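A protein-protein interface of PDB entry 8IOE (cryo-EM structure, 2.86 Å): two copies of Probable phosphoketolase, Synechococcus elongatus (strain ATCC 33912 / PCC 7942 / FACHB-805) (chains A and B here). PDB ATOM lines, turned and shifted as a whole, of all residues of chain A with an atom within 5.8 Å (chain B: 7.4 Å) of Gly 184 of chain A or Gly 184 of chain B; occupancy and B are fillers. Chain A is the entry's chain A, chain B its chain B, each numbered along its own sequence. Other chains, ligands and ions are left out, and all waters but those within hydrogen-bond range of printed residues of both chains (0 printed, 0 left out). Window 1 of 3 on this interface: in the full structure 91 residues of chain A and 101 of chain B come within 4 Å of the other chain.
O of Glu 182 of chain A lies within hydrogen-bond range of OG1 of Thr 188 of chain B, 2.7 Å away. The backbone NH of Ser 469 of chain B sits at hydrogen-bond distance from the side-chain carboxylate of Glu 182 of chain A, at 3.0 Å. The side-chain hydroxyl (OG1) of Thr 188 of chain B lies close to the backbone carbonyl oxygen (O) of Thr 183 of chain A (3.2 Å). The backbone NH (N) of Gly 184 of chain A lies within hydrogen-bond range of the side-chain hydroxyl (OG1) of Thr 188 of chain B. The side-chain hydroxyl (OG1) of Thr 188 of chain A lies within hydrogen-bond range of the backbone carbonyl oxygen (O) of Glu 182 of chain B (3.0 Å). The side-chain hydroxyl of Thr 188 of chain A lies within hydrogen-bond range of the backbone carbonyl oxygen of Thr 183 of chain B (3.5 Å). N of Gly 184 of chain B lies close to OG1 of Thr 188 of chain A, 3.4 Å away.
The side-chain hydroxyl (OG) of Ser 469 of chain A sits close to the backbone NH (N) of His 471 of chain A, at 3.4 Å. O of Glu 180 of chain B lies within hydrogen-bond range of OG1 of Thr 183 of chain B (2.5 Å).
Among the printed residues, pairs that only touch across the chains: Glu 182 of chain A with Leu 468 of chain B (3.2 Å), Gly 184 of chain A with Gly 184 of chain B (3.3 Å), Ala 187 of chain A with Ala 187 of chain B (3.7 Å), Ala 187 of chain A with Thr 188 of chain B (3.5 Å), Thr 188 of chain A with Ala 187 of chain B (3.8 Å), Ser 469 of chain A with Glu 182 of chain B (3.2 Å) and Ser 469 of chain A with Gly 184 of chain B (3.98 Å).
Gly 184 of chain A touches two residues of chain B. Of the printed residues of chain A, Gly 184 of chain B touches Gly 184 (3.3 Å), Thr 188 (3.3 Å) and Ser 469 (3.98 Å). Of the printed residues of chain A, Ser 469 of chain B touches Glu 182 (3.0 Å). Printed residues of chain B within 4 Å of Ser 469 of chain A: Glu 182 (3.2 Å) and Gly 184 (3.98 Å). Leu 186 of chain A touches none of the printed residues of chain B. The nearest residue of chain B that does not touch Gly 184 of chain A is Ser 469 of chain B (4.1 Å). The nearest printed residue of chain A that does not touch Gly 184 of chain B is Pro 185 of chain A (4.5 Å).
Of the 19 printed residues of chain B, 7 touch a printed residue of chain A. Along chain A the printed residues that touch a printed residue of chain B span positions 182 to 469. Among the printed residues, no Asp or Glu carboxylate lies within 4 Å of a Lys or Arg side-chain nitrogen of the other chain.
Thr 183 of chain A touches Thr 188 of chain B, and with the chains exchanged Thr 188 of chain A touches Thr 183 of chain B. Gly 184 of chain A touches its own counterpart, Gly 184 of chain B. Gly 184 of chain A touches Thr 188 of chain B, and with the chains exchanged Thr 188 of chain A touches Gly 184 of chain B. Ala 187 of chain A touches Thr 188 of chain B, and with the chains exchanged Thr 188 of chain A touches Ala 187 of chain B. Positions printed for both chains: 182, 183, 184, 185, 186, 187, 188, 189, 469 and 471. Of the 14 pairs that touch across the chains among the printed residues, 12 have their exchanged pair printed and touching as well.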
ATOM      1  N   GLU A 182      -5.324   9.306 -20.937  1.00  0.00           N
ATOM      2  CA  GLU A 182      -5.679  10.406 -21.818  1.00  0.00           C
ATOM      3  C   GLU A 182      -6.066   9.950 -23.220  1.00  0.00           C
ATOM      4  O   GLU A 182      -6.548  10.773 -24.005  1.00  0.00           O
ATOM      5  CB  GLU A 182      -4.521  11.404 -21.894  1.00  0.00           C
ATOM      6  CG  GLU A 182      -3.259  10.847 -22.523  1.00  0.00           C
ATOM      7  CD  GLU A 182      -3.253  10.996 -24.028  1.00  0.00           C
ATOM      8  OE1 GLU A 182      -3.499  12.119 -24.505  1.00  0.00           O
ATOM      9  OE2 GLU A 182      -3.045   9.986 -24.730  1.00  0.00           O
ATOM     10  N   THR A 183      -5.854   8.681 -23.558  1.00  0.00           N
ATOM     11  CA  THR A 183      -6.159   8.203 -24.899  1.00  0.00           C
ATOM     12  C   THR A 183      -7.666   8.200 -25.145  1.00  0.00           C
ATOM     13  O   THR A 183      -8.478   8.174 -24.217  1.00  0.00           O
ATOM     14  CB  THR A 183      -5.598   6.799 -25.117  1.00  0.00           C
ATOM     15  OG1 THR A 183      -6.055   5.931 -24.074  1.00  0.00           O
ATOM     16  CG2 THR A 183      -4.083   6.827 -25.120  1.00  0.00           C
ATOM     17  N   GLY A 184      -8.028   8.230 -26.425  1.00  0.00           N
ATOM     18  CA  GLY A 184      -9.410   8.277 -26.845  1.00  0.00           C
ATOM     19  C   GLY A 184     -10.267   7.124 -26.358  1.00  0.00           C
ATOM     20  O   GLY A 184     -11.334   7.333 -25.773  1.00  0.00           O
ATOM     21  N   PRO A 185      -9.833   5.884 -26.604  1.00  0.00           N
ATOM     22  CA  PRO A 185     -10.589   4.736 -26.080  1.00  0.00           C
ATOM     23  C   PRO A 185     -10.732   4.722 -24.570  1.00  0.00           C
ATOM     24  O   PRO A 185     -11.746   4.229 -24.062  1.00  0.00           O
ATOM     25  CB  PRO A 185      -9.776   3.538 -26.579  1.00  0.00           C
ATOM     26  CG  PRO A 185      -9.193   4.015 -27.848  1.00  0.00           C
ATOM     27  CD  PRO A 185      -8.863   5.464 -27.632  1.00  0.00           C
ATOM     28  N   LEU A 186      -9.752   5.235 -23.828  1.00  0.00           N
ATOM     29  CA  LEU A 186      -9.887   5.250 -22.379  1.00  0.00           C
ATOM     30  C   LEU A 186     -10.633   6.485 -21.888  1.00  0.00           C
ATOM     31  O   LEU A 186     -11.232   6.450 -20.808  1.00  0.00           O
ATOM     32  CB  LEU A 186      -8.511   5.155 -21.720  1.00  0.00           C
ATOM     33  CG  LEU A 186      -8.476   4.832 -20.224  1.00  0.00           C
ATOM     34  CD1 LEU A 186      -9.608   3.929 -19.840  1.00  0.00           C
ATOM     35  CD2 LEU A 186      -7.182   4.153 -19.874  1.00  0.00           C
ATOM     36  N   ALA A 187     -10.620   7.574 -22.656  1.00  0.00           N
ATOM     37  CA  ALA A 187     -11.383   8.752 -22.259  1.00  0.00           C
ATOM     38  C   ALA A 187     -12.877   8.456 -22.240  1.00  0.00           C
ATOM     39  O   ALA A 187     -13.596   8.902 -21.340  1.00  0.00           O
ATOM     40  CB  ALA A 187     -11.076   9.918 -23.197  1.00  0.00           C
ATOM     41  N   THR A 188     -13.359   7.694 -23.220  1.00  0.00           N
ATOM     42  CA  THR A 188     -14.769   7.325 -23.269  1.00  0.00           C
ATOM     43  C   THR A 188     -15.114   6.224 -22.274  1.00  0.00           C
ATOM     44  O   THR A 188     -16.189   6.261 -21.663  1.00  0.00           O
ATOM     45  CB  THR A 188     -15.133   6.890 -24.692  1.00  0.00           C
ATOM     46  OG1 THR A 188     -15.053   8.018 -25.571  1.00  0.00           O
ATOM     47  CG2 THR A 188     -16.536   6.310 -24.751  1.00  0.00           C
ATOM     48  N   SER A 189     -14.199   5.276 -22.054  1.00  0.00           N
ATOM     49  CA  SER A 189     -14.523   4.052 -21.327  1.00  0.00           C
ATOM     50  C   SER A 189     -14.896   4.302 -19.873  1.00  0.00           C
ATOM     51  O   SER A 189     -15.407   3.389 -19.216  1.00  0.00           O
ATOM     52  CB  SER A 189     -13.350   3.076 -21.392  1.00  0.00           C
ATOM     53  OG  SER A 189     -13.089   2.684 -22.727  1.00  0.00           O
ATOM     54  N   SER A 469     -19.290   4.990 -29.301  1.00  0.00           N
ATOM     55  CA  SER A 469     -17.877   4.645 -29.415  1.00  0.00           C
ATOM     56  C   SER A 469     -17.729   3.147 -29.627  1.00  0.00           C
ATOM     57  O   SER A 469     -18.051   2.352 -28.739  1.00  0.00           O
ATOM     58  CB  SER A 469     -17.119   5.091 -28.170  1.00  0.00           C
ATOM     59  OG  SER A 469     -15.797   4.579 -28.176  1.00  0.00           O
ATOM     60  N   HIS A 471     -14.915   1.715 -29.813  1.00  0.00           N
ATOM     61  CA  HIS A 471     -13.774   1.279 -29.015  1.00  0.00           C
ATOM     62  C   HIS A 471     -14.235   0.599 -27.734  1.00  0.00           C
ATOM     63  O   HIS A 471     -13.718  -0.457 -27.354  1.00  0.00           O
ATOM     64  CB  HIS A 471     -12.871   2.467 -28.694  1.00  0.00           C
ATOM     65  CG  HIS A 471     -12.243   3.091 -29.900  1.00  0.00           C
ATOM     66  ND1 HIS A 471     -11.245   2.475 -30.622  1.00  0.00           N
ATOM     67  CD2 HIS A 471     -12.465   4.282 -30.503  1.00  0.00           C
ATOM     68  CE1 HIS A 471     -10.882   3.257 -31.622  1.00  0.00           C
ATOM     69  NE2 HIS A 471     -11.606   4.361 -31.571  1.00  0.00           N
ATOM     70  N   LEU B 153     -17.577  10.950 -37.452  1.00  0.00           N
ATOM     71  CA  LEU B 153     -17.970  11.758 -36.307  1.00  0.00           C
ATOM     72  C   LEU B 153     -16.944  11.588 -35.193  1.00  0.00           C
ATOM     73  O   LEU B 153     -16.655  10.461 -34.776  1.00  0.00           O
ATOM     74  CB  LEU B 153     -19.368  11.367 -35.827  1.00  0.00           C
ATOM     75  CG  LEU B 153     -20.592  12.029 -36.479  1.00  0.00           C
ATOM     76  CD1 LEU B 153     -20.645  13.500 -36.141  1.00  0.00           C
ATOM     77  CD2 LEU B 153     -20.628  11.858 -37.985  1.00  0.00           C
ATOM     78  N   GLY B 154     -16.398  12.704 -34.718  1.00  0.00           N
ATOM     79  CA  GLY B 154     -15.480  12.681 -33.598  1.00  0.00           C
ATOM     80  C   GLY B 154     -14.198  13.445 -33.842  1.00  0.00           C
ATOM     81  O   GLY B 154     -13.430  13.696 -32.909  1.00  0.00           O
ATOM     82  N   TYR B 155     -13.956  13.825 -35.094  1.00  0.00           N
ATOM     83  CA  TYR B 155     -12.708  14.465 -35.486  1.00  0.00           C
ATOM     84  C   TYR B 155     -12.862  15.962 -35.694  1.00  0.00           C
ATOM     85  O   TYR B 155     -11.925  16.611 -36.170  1.00  0.00           O
ATOM     86  CB  TYR B 155     -12.161  13.827 -36.766  1.00  0.00           C
ATOM     87  CG  TYR B 155     -12.063  12.315 -36.755  1.00  0.00           C
ATOM     88  CD1 TYR B 155     -11.931  11.607 -35.568  1.00  0.00           C
ATOM     89  CD2 TYR B 155     -12.099  11.597 -37.941  1.00  0.00           C
ATOM     90  CE1 TYR B 155     -11.845  10.232 -35.564  1.00  0.00           C
ATOM     91  CE2 TYR B 155     -12.010  10.222 -37.945  1.00  0.00           C
ATOM     92  CZ  TYR B 155     -11.882   9.544 -36.754  1.00  0.00           C
ATOM     93  OH  TYR B 155     -11.793   8.173 -36.750  1.00  0.00           O
ATOM     94  N   GLU B 180     -22.035  12.666 -31.070  1.00  0.00           N
ATOM     95  CA  GLU B 180     -20.634  12.659 -31.474  1.00  0.00           C
ATOM     96  C   GLU B 180     -19.702  12.634 -30.269  1.00  0.00           C
ATOM     97  O   GLU B 180     -18.603  12.073 -30.348  1.00  0.00           O
ATOM     98  CB  GLU B 180     -20.345  13.882 -32.344  1.00  0.00           C
ATOM     99  CG  GLU B 180     -18.967  13.902 -32.974  1.00  0.00           C
ATOM    100  CD  GLU B 180     -18.682  15.196 -33.708  1.00  0.00           C
ATOM    101  OE1 GLU B 180     -19.560  16.085 -33.716  1.00  0.00           O
ATOM    102  OE2 GLU B 180     -17.576  15.326 -34.277  1.00  0.00           O
ATOM    103  N   ALA B 181     -20.125  13.221 -29.149  1.00  0.00           N
ATOM    104  CA  ALA B 181     -19.262  13.326 -27.979  1.00  0.00           C
ATOM    105  C   ALA B 181     -18.994  11.983 -27.320  1.00  0.00           C
ATOM    106  O   ALA B 181     -18.070  11.883 -26.506  1.00  0.00           O
ATOM    107  CB  ALA B 181     -19.869  14.293 -26.966  1.00  0.00           C
ATOM    108  N   GLU B 182     -19.776  10.952 -27.639  1.00  0.00           N
ATOM    109  CA  GLU B 182     -19.477   9.623 -27.125  1.00  0.00           C
ATOM    110  C   GLU B 182     -18.229   9.024 -27.760  1.00  0.00           C
ATOM    111  O   GLU B 182     -17.624   8.126 -27.169  1.00  0.00           O
ATOM    112  CB  GLU B 182     -20.655   8.681 -27.349  1.00  0.00           C
ATOM    113  CG  GLU B 182     -21.842   8.904 -26.437  1.00  0.00           C
ATOM    114  CD  GLU B 182     -22.865   7.790 -26.553  1.00  0.00           C
ATOM    115  OE1 GLU B 182     -22.566   6.771 -27.205  1.00  0.00           O
ATOM    116  OE2 GLU B 182     -23.971   7.930 -25.998  1.00  0.00           O
ATOM    117  N   THR B 183     -17.839   9.492 -28.942  1.00  0.00           N
ATOM    118  CA  THR B 183     -16.684   8.931 -29.626  1.00  0.00           C
ATOM    119  C   THR B 183     -15.400   9.221 -28.856  1.00  0.00           C
ATOM    120  O   THR B 183     -15.246  10.270 -28.227  1.00  0.00           O
ATOM    121  CB  THR B 183     -16.575   9.489 -31.043  1.00  0.00           C
ATOM    122  OG1 THR B 183     -16.531  10.920 -30.992  1.00  0.00           O
ATOM    123  CG2 THR B 183     -17.766   9.056 -31.875  1.00  0.00           C
ATOM    124  N   GLY B 184     -14.479   8.265 -28.909  1.00  0.00           N
ATOM    125  CA  GLY B 184     -13.206   8.369 -28.233  1.00  0.00           C
ATOM    126  C   GLY B 184     -12.334   9.537 -28.657  1.00  0.00           C
ATOM    127  O   GLY B 184     -11.808  10.265 -27.811  1.00  0.00           O
ATOM    128  N   PRO B 185     -12.143   9.733 -29.967  1.00  0.00           N
ATOM    129  CA  PRO B 185     -11.354  10.891 -30.415  1.00  0.00           C
ATOM    130  C   PRO B 185     -11.902  12.234 -29.968  1.00  0.00           C
ATOM    131  O   PRO B 185     -11.118  13.160 -29.733  1.00  0.00           O
ATOM    132  CB  PRO B 185     -11.383  10.752 -31.941  1.00  0.00           C
ATOM    133  CG  PRO B 185     -11.437   9.298 -32.154  1.00  0.00           C
ATOM    134  CD  PRO B 185     -12.307   8.752 -31.057  1.00  0.00           C
ATOM    135  N   LEU B 186     -13.220  12.381 -29.847  1.00  0.00           N
ATOM    136  CA  LEU B 186     -13.756  13.655 -29.388  1.00  0.00           C
ATOM    137  C   LEU B 186     -13.585  13.843 -27.887  1.00  0.00           C
ATOM    138  O   LEU B 186     -13.369  14.970 -27.432  1.00  0.00           O
ATOM    139  CB  LEU B 186     -15.229  13.779 -29.771  1.00  0.00           C
ATOM    140  CG  LEU B 186     -15.862  15.140 -29.487  1.00  0.00           C
ATOM    141  CD1 LEU B 186     -14.961  16.243 -29.955  1.00  0.00           C
ATOM    142  CD2 LEU B 186     -17.184  15.255 -30.188  1.00  0.00           C
ATOM    143  N   ALA B 187     -13.673  12.762 -27.108  1.00  0.00           N
ATOM    144  CA  ALA B 187     -13.534  12.884 -25.661  1.00  0.00           C
ATOM    145  C   ALA B 187     -12.144  13.376 -25.277  1.00  0.00           C
ATOM    146  O   ALA B 187     -12.000  14.226 -24.392  1.00  0.00           O
ATOM    147  CB  ALA B 187     -13.837  11.545 -24.993  1.00  0.00           C
ATOM    148  N   THR B 188     -11.110  12.859 -25.938  1.00  0.00           N
ATOM    149  CA  THR B 188      -9.750  13.304 -25.656  1.00  0.00           C
ATOM    150  C   THR B 188      -9.501  14.720 -26.161  1.00  0.00           C
ATOM    151  O   THR B 188      -8.822  15.506 -25.490  1.00  0.00           O
ATOM    152  CB  THR B 188      -8.753  12.319 -26.274  1.00  0.00           C
ATOM    153  OG1 THR B 188      -8.745  11.112 -25.504  1.00  0.00           O
ATOM    154  CG2 THR B 188      -7.350  12.893 -26.306  1.00  0.00           C
ATOM    155  N   SER B 189     -10.091  15.084 -27.302  1.00  0.00           N
ATOM    156  CA  SER B 189      -9.784  16.343 -27.970  1.00  0.00           C
ATOM    157  C   SER B 189     -10.183  17.568 -27.162  1.00  0.00           C
ATOM    158  O   SER B 189      -9.789  18.679 -27.530  1.00  0.00           O
ATOM    159  CB  SER B 189     -10.468  16.393 -29.335  1.00  0.00           C
ATOM    160  OG  SER B 189      -9.993  15.361 -30.180  1.00  0.00           O
ATOM    161  N   TRP B 190     -10.968  17.402 -26.096  1.00  0.00           N
ATOM    162  CA  TRP B 190     -11.297  18.534 -25.238  1.00  0.00           C
ATOM    163  C   TRP B 190     -10.049  19.108 -24.580  1.00  0.00           C
ATOM    164  O   TRP B 190      -9.915  20.329 -24.445  1.00  0.00           O
ATOM    165  CB  TRP B 190     -12.312  18.111 -24.181  1.00  0.00           C
ATOM    166  CG  TRP B 190     -13.640  17.742 -24.745  1.00  0.00           C
ATOM    167  CD1 TRP B 190     -14.163  16.491 -24.852  1.00  0.00           C
ATOM    168  CD2 TRP B 190     -14.617  18.635 -25.286  1.00  0.00           C
ATOM    169  NE1 TRP B 190     -15.410  16.548 -25.424  1.00  0.00           N
ATOM    170  CE2 TRP B 190     -15.711  17.855 -25.699  1.00  0.00           C
ATOM    171  CE3 TRP B 190     -14.673  20.020 -25.461  1.00  0.00           C
ATOM    172  CZ2 TRP B 190     -16.847  18.411 -26.276  1.00  0.00           C
ATOM    173  CZ3 TRP B 190     -15.801  20.570 -26.033  1.00  0.00           C
ATOM    174  CH2 TRP B 190     -16.872  19.767 -26.435  1.00  0.00           C
ATOM    175  N   LEU B 468       0.381  11.718 -26.506  1.00  0.00           N
ATOM    176  CA  LEU B 468       0.465  10.353 -27.013  1.00  0.00           C
ATOM    177  C   LEU B 468      -0.851   9.832 -27.576  1.00  0.00           C
ATOM    178  O   LEU B 468      -0.876   8.716 -28.104  1.00  0.00           O
ATOM    179  CB  LEU B 468       0.966   9.400 -25.924  1.00  0.00           C
ATOM    180  CG  LEU B 468       0.011   9.037 -24.790  1.00  0.00           C
ATOM    181  CD1 LEU B 468       0.307   7.643 -24.273  1.00  0.00           C
ATOM    182  CD2 LEU B 468       0.124  10.045 -23.671  1.00  0.00           C
ATOM    183  N   SER B 469      -1.935  10.593 -27.481  1.00  0.00           N
ATOM    184  CA  SER B 469      -3.178  10.235 -28.159  1.00  0.00           C
ATOM    185  C   SER B 469      -3.020  10.588 -29.630  1.00  0.00           C
ATOM    186  O   SER B 469      -3.093  11.758 -30.010  1.00  0.00           O
ATOM    187  CB  SER B 469      -4.366  10.959 -27.541  1.00  0.00           C
ATOM    188  OG  SER B 469      -5.509  10.855 -28.371  1.00  0.00           O
ATOM    189  N   GLU B 470      -2.795   9.572 -30.467  1.00  0.00           N
ATOM    190  CA  GLU B 470      -2.567   9.819 -31.885  1.00  0.00           C
ATOM    191  C   GLU B 470      -3.804  10.348 -32.593  1.00  0.00           C
ATOM    192  O   GLU B 470      -3.677  10.929 -33.675  1.00  0.00           O
ATOM    193  CB  GLU B 470      -2.088   8.546 -32.580  1.00  0.00           C
ATOM    194  CG  GLU B 470      -0.695   8.107 -32.175  1.00  0.00           C
ATOM    195  CD  GLU B 470      -0.092   7.123 -33.157  1.00  0.00           C
ATOM    196  OE1 GLU B 470      -0.678   6.931 -34.243  1.00  0.00           O
ATOM    197  OE2 GLU B 470       0.970   6.545 -32.846  1.00  0.00           O
ATOM    198  N   HIS B 471      -4.991  10.151 -32.020  1.00  0.00           N
ATOM    199  CA  HIS B 471      -6.206  10.674 -32.635  1.00  0.00           C
ATOM    200  C   HIS B 471      -6.178  12.195 -32.696  1.00  0.00           C
ATOM    201  O   HIS B 471      -6.142  12.788 -33.778  1.00  0.00           O
ATOM    202  CB  HIS B 471      -7.434  10.191 -31.865  1.00  0.00           C
ATOM    203  CG  HIS B 471      -7.733   8.738 -32.054  1.00  0.00           C
ATOM    204  ND1 HIS B 471      -8.129   8.213 -33.264  1.00  0.00           N
ATOM    205  CD2 HIS B 471      -7.704   7.703 -31.184  1.00  0.00           C
ATOM    206  CE1 HIS B 471      -8.326   6.913 -33.133  1.00  0.00           C
ATOM    207  NE2 HIS B 471      -8.076   6.579 -31.881  1.00  0.00           N
ATOM    208  N   THR B 472      -6.169  12.843 -31.531  1.00  0.00           N
ATOM    209  CA  THR B 472      -6.194  14.299 -31.503  1.00  0.00           C
ATOM    210  C   THR B 472      -4.931  14.897 -32.098  1.00  0.00           C
ATOM    211  O   THR B 472      -4.969  16.007 -32.639  1.00  0.00           O
ATOM    212  CB  THR B 472      -6.385  14.794 -30.072  1.00  0.00           C
ATOM    213  OG1 THR B 472      -6.199  16.214 -30.030  1.00  0.00           O
ATOM    214  CG2 THR B 472      -5.387  14.127 -29.145  1.00  0.00           C
